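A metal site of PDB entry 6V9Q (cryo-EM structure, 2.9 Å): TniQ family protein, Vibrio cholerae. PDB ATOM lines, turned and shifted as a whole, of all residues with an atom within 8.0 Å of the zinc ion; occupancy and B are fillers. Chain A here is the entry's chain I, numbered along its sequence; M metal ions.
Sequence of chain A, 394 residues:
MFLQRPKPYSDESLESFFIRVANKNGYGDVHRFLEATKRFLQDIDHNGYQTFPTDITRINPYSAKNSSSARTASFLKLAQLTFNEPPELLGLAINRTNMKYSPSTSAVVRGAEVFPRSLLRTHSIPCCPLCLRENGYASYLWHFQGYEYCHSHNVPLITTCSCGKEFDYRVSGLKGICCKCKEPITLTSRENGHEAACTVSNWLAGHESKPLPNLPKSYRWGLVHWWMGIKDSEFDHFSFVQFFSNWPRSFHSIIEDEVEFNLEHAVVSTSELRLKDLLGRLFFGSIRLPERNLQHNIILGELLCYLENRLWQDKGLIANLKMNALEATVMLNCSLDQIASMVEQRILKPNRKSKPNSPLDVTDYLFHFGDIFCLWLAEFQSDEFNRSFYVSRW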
ATOM      1  N   THR A 160      17.943  -1.627 -26.565  1.00  0.00           N
ATOM      2  CA  THR A 160      16.502  -1.448 -26.455  1.00  0.00           C
ATOM      3  C   THR A 160      15.960  -2.485 -25.493  1.00  0.00           C
ATOM      4  O   THR A 160      16.312  -3.666 -25.583  1.00  0.00           O
ATOM      5  CB  THR A 160      15.824  -1.559 -27.831  1.00  0.00           C
ATOM      6  OG1 THR A 160      16.373  -0.593 -28.733  1.00  0.00           O
ATOM      7  CG2 THR A 160      14.331  -1.339 -27.736  1.00  0.00           C
ATOM      8  N   CYS A 161      15.104  -2.050 -24.569  1.00  0.00           N
ATOM      9  CA  CYS A 161      14.452  -2.962 -23.643  1.00  0.00           C
ATOM     10  C   CYS A 161      13.334  -3.741 -24.348  1.00  0.00           C
ATOM     11  O   CYS A 161      13.078  -3.577 -25.542  1.00  0.00           O
ATOM     12  CB  CYS A 161      13.904  -2.201 -22.434  1.00  0.00           C
ATOM     13  SG  CYS A 161      13.087  -3.243 -21.201  1.00  0.00           S
ATOM     14  N   SER A 162      12.651  -4.596 -23.584  1.00  0.00           N
ATOM     15  CA  SER A 162      11.560  -5.385 -24.149  1.00  0.00           C
ATOM     16  C   SER A 162      10.314  -4.552 -24.407  1.00  0.00           C
ATOM     17  O   SER A 162       9.456  -4.973 -25.185  1.00  0.00           O
ATOM     18  CB  SER A 162      11.220  -6.546 -23.217  1.00  0.00           C
ATOM     19  OG  SER A 162      12.293  -7.462 -23.133  1.00  0.00           O
ATOM     20  N   CYS A 163      10.196  -3.385 -23.775  1.00  0.00           N
ATOM     21  CA  CYS A 163       9.054  -2.507 -23.986  1.00  0.00           C
ATOM     22  C   CYS A 163       9.323  -1.434 -25.033  1.00  0.00           C
ATOM     23  O   CYS A 163       8.625  -0.407 -25.069  1.00  0.00           O
ATOM     24  CB  CYS A 163       8.637  -1.856 -22.662  1.00  0.00           C
ATOM     25  SG  CYS A 163       7.974  -3.037 -21.463  1.00  0.00           S
ATOM     26  N   GLY A 164      10.331  -1.636 -25.890  1.00  0.00           N
ATOM     27  CA  GLY A 164      10.627  -0.708 -26.953  1.00  0.00           C
ATOM     28  C   GLY A 164      11.480   0.485 -26.571  1.00  0.00           C
ATOM     29  O   GLY A 164      11.931   1.206 -27.462  1.00  0.00           O
ATOM     30  N   LYS A 165      11.709   0.716 -25.290  1.00  0.00           N
ATOM     31  CA  LYS A 165      12.478   1.863 -24.835  1.00  0.00           C
ATOM     32  C   LYS A 165      13.961   1.533 -24.814  1.00  0.00           C
ATOM     33  O   LYS A 165      14.359   0.408 -24.530  1.00  0.00           O
ATOM     34  CB  LYS A 165      12.029   2.301 -23.440  1.00  0.00           C
ATOM     35  CG  LYS A 165      10.599   2.784 -23.386  1.00  0.00           C
ATOM     36  CD  LYS A 165      10.420   4.046 -24.201  1.00  0.00           C
ATOM     37  CE  LYS A 165      11.095   5.233 -23.534  1.00  0.00           C
ATOM     38  NZ  LYS A 165      10.861   6.503 -24.283  1.00  0.00           N
ATOM     39  N   GLU A 166      14.780   2.536 -25.137  1.00  0.00           N
ATOM     40  CA  GLU A 166      16.215   2.368 -25.056  1.00  0.00           C
ATOM     41  C   GLU A 166      16.677   2.415 -23.608  1.00  0.00           C
ATOM     42  O   GLU A 166      15.959   2.901 -22.719  1.00  0.00           O
ATOM     43  CB  GLU A 166      16.940   3.440 -25.874  1.00  0.00           C
ATOM     44  CG  GLU A 166      16.780   4.847 -25.311  1.00  0.00           C
ATOM     45  CD  GLU A 166      17.504   5.884 -26.144  1.00  0.00           C
ATOM     46  OE1 GLU A 166      18.105   5.507 -27.168  1.00  0.00           O
ATOM     47  OE2 GLU A 166      17.489   7.068 -25.755  1.00  0.00           O
ATOM     48  N   PHE A 167      17.879   1.907 -23.367  1.00  0.00           N
ATOM     49  CA  PHE A 167      18.482   1.922 -22.042  1.00  0.00           C
ATOM     50  C   PHE A 167      19.880   2.522 -22.160  1.00  0.00           C
ATOM     51  O   PHE A 167      20.792   1.879 -22.687  1.00  0.00           O
ATOM     52  CB  PHE A 167      18.544   0.519 -21.433  1.00  0.00           C
ATOM     53  CG  PHE A 167      19.130   0.495 -20.053  1.00  0.00           C
ATOM     54  CD1 PHE A 167      18.390   0.899 -18.964  1.00  0.00           C
ATOM     55  CD2 PHE A 167      20.429   0.071 -19.853  1.00  0.00           C
ATOM     56  CE1 PHE A 167      18.937   0.875 -17.692  1.00  0.00           C
ATOM     57  CE2 PHE A 167      20.988   0.044 -18.588  1.00  0.00           C
ATOM     58  CZ  PHE A 167      20.231   0.449 -17.501  1.00  0.00           C
ATOM     59  N   ILE A 177      18.053  -1.291 -14.475  1.00  0.00           N
ATOM     60  CA  ILE A 177      16.604  -1.186 -14.367  1.00  0.00           C
ATOM     61  C   ILE A 177      16.120  -0.184 -15.402  1.00  0.00           C
ATOM     62  O   ILE A 177      16.633   0.940 -15.477  1.00  0.00           O
ATOM     63  CB  ILE A 177      16.180  -0.759 -12.949  1.00  0.00           C
ATOM     64  CG1 ILE A 177      16.707  -1.748 -11.919  1.00  0.00           C
ATOM     65  CG2 ILE A 177      14.668  -0.645 -12.841  1.00  0.00           C
ATOM     66  CD1 ILE A 177      16.191  -3.150 -12.095  1.00  0.00           C
ATOM     67  N   CYS A 178      15.132  -0.585 -16.204  1.00  0.00           N
ATOM     68  CA  CYS A 178      14.594   0.271 -17.254  1.00  0.00           C
ATOM     69  C   CYS A 178      13.831   1.448 -16.659  1.00  0.00           C
ATOM     70  O   CYS A 178      13.530   1.505 -15.462  1.00  0.00           O
ATOM     71  CB  CYS A 178      13.695  -0.541 -18.188  1.00  0.00           C
ATOM     72  SG  CYS A 178      12.992   0.404 -19.566  1.00  0.00           S
ATOM     73  N   CYS A 179      13.497   2.416 -17.525  1.00  0.00           N
ATOM     74  CA  CYS A 179      12.819   3.621 -17.057  1.00  0.00           C
ATOM     75  C   CYS A 179      11.300   3.511 -17.176  1.00  0.00           C
ATOM     76  O   CYS A 179      10.593   3.954 -16.271  1.00  0.00           O
ATOM     77  CB  CYS A 179      13.316   4.835 -17.846  1.00  0.00           C
ATOM     78  SG  CYS A 179      15.043   5.246 -17.543  1.00  0.00           S
ATOM     79  N   LYS A 180      10.804   2.940 -18.264  1.00  0.00           N
ATOM     80  CA  LYS A 180       9.361   2.847 -18.455  1.00  0.00           C
ATOM     81  C   LYS A 180       8.758   1.719 -17.637  1.00  0.00           C
ATOM     82  O   LYS A 180       7.853   1.951 -16.825  1.00  0.00           O
ATOM     83  CB  LYS A 180       9.042   2.667 -19.944  1.00  0.00           C
ATOM     84  CG  LYS A 180       7.545   2.649 -20.252  1.00  0.00           C
ATOM     85  CD  LYS A 180       7.291   2.577 -21.746  1.00  0.00           C
ATOM     86  CE  LYS A 180       5.801   2.410 -22.046  1.00  0.00           C
ATOM     87  NZ  LYS A 180       5.019   3.609 -21.646  1.00  0.00           N
ATOM     88  N   CYS A 181       9.242   0.498 -17.831  1.00  0.00           N
ATOM     89  CA  CYS A 181       8.656  -0.672 -17.179  1.00  0.00           C
ATOM     90  C   CYS A 181       9.261  -0.975 -15.814  1.00  0.00           C
ATOM     91  O   CYS A 181       8.753  -1.869 -15.133  1.00  0.00           O
ATOM     92  CB  CYS A 181       8.814  -1.904 -18.079  1.00  0.00           C
ATOM     93  SG  CYS A 181      10.519  -2.423 -18.347  1.00  0.00           S
ATOM     94  N   LYS A 182      10.302  -0.232 -15.411  1.00  0.00           N
ATOM     95  CA  LYS A 182      11.153  -0.419 -14.220  1.00  0.00           C
ATOM     96  C   LYS A 182      11.500  -1.877 -13.921  1.00  0.00           C
ATOM     97  O   LYS A 182      11.521  -2.303 -12.762  1.00  0.00           O
ATOM     98  CB  LYS A 182      10.551   0.296 -12.992  1.00  0.00           C
ATOM     99  CG  LYS A 182       9.188  -0.141 -12.459  1.00  0.00           C
ATOM    100  CD  LYS A 182       8.764   0.706 -11.273  1.00  0.00           C
ATOM    101  CE  LYS A 182       7.415   0.264 -10.724  1.00  0.00           C
ATOM    102  NZ  LYS A 182       6.996   1.081  -9.557  1.00  0.00           N
ATOM    103  N   GLU A 183      11.821  -2.637 -14.960  1.00  0.00           N
ATOM    104  CA  GLU A 183      12.203  -4.029 -14.875  1.00  0.00           C
ATOM    105  C   GLU A 183      13.601  -4.231 -15.440  1.00  0.00           C
ATOM    106  O   GLU A 183      14.074  -3.426 -16.246  1.00  0.00           O
ATOM    107  CB  GLU A 183      11.209  -4.927 -15.636  1.00  0.00           C
ATOM    108  CG  GLU A 183       9.821  -4.993 -15.013  1.00  0.00           C
ATOM    109  CD  GLU A 183       9.817  -5.698 -13.665  1.00  0.00           C
ATOM    110  OE1 GLU A 183      10.634  -6.624 -13.475  1.00  0.00           O
ATOM    111  OE2 GLU A 183       9.004  -5.323 -12.811  1.00  0.00           O
ATOM    112  N   PRO A 184      14.315  -5.279 -15.005  1.00  0.00           N
ATOM    113  CA  PRO A 184      15.569  -5.637 -15.673  1.00  0.00           C
ATOM    114  C   PRO A 184      15.325  -6.081 -17.107  1.00  0.00           C
ATOM    115  O   PRO A 184      14.302  -6.706 -17.419  1.00  0.00           O
ATOM    116  CB  PRO A 184      16.112  -6.783 -14.817  1.00  0.00           C
ATOM    117  CG  PRO A 184      15.505  -6.561 -13.467  1.00  0.00           C
ATOM    118  CD  PRO A 184      14.137  -6.008 -13.739  1.00  0.00           C
ATOM    119  N   ILE A 185      16.269  -5.760 -17.980  1.00  0.00           N
ATOM    120  CA  ILE A 185      16.090  -5.980 -19.412  1.00  0.00           C
ATOM    121  C   ILE A 185      16.438  -7.429 -19.744  1.00  0.00           C
ATOM    122  O   ILE A 185      17.506  -7.925 -19.367  1.00  0.00           O
ATOM    123  CB  ILE A 185      16.946  -5.005 -20.236  1.00  0.00           C
ATOM    124  CG1 ILE A 185      16.560  -3.538 -19.958  1.00  0.00           C
ATOM    125  CG2 ILE A 185      16.811  -5.275 -21.729  1.00  0.00           C
ATOM    126  CD1 ILE A 185      17.465  -2.822 -18.969  1.00  0.00           C
ATOM    127  N   THR A 186      15.536  -8.104 -20.448  1.00  0.00           N
ATOM    128  CA  THR A 186      15.791  -9.452 -20.927  1.00  0.00           C
ATOM    129  C   THR A 186      16.846  -9.414 -22.035  1.00  0.00           C
ATOM    130  O   THR A 186      16.842  -8.511 -22.879  1.00  0.00           O
ATOM    131  CB  THR A 186      14.489 -10.080 -21.441  1.00  0.00           C
ATOM    132  OG1 THR A 186      13.485  -9.974 -20.421  1.00  0.00           O
ATOM    133  CG2 THR A 186      14.675 -11.554 -21.766  1.00  0.00           C
HETATM  134 ZN    ZN M   1      11.484  -1.387 -20.461  1.00  0.00          ZN
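Merely in contact with the zinc ion: Cys 163 (3.6 Å). Four residues have an atom within 4 Å of the zinc ion: Cys 161, Cys 163, Cys 178 and Cys 181. The nearest printed residue that does not touch the zinc ion is Ser 162 (4.6 Å).
N of Lys 180 sits close to SG of Cys 178 (3.6 Å). N of Cys 178 is in hydrogen-bond range of O of Glu 183 (3.0 Å). SG of Cys 181 sits close to N of Glu 183, 3.6 Å away.
The side-chain sulfur (SG) of Cys 178 binds the zinc ion, at 2.5 Å. The zinc ion is bound by SG of Cys 181, 2.5 Å away. The zinc ion is bound by SG of Cys 161. The zinc ion has three donor atoms within binding distance.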
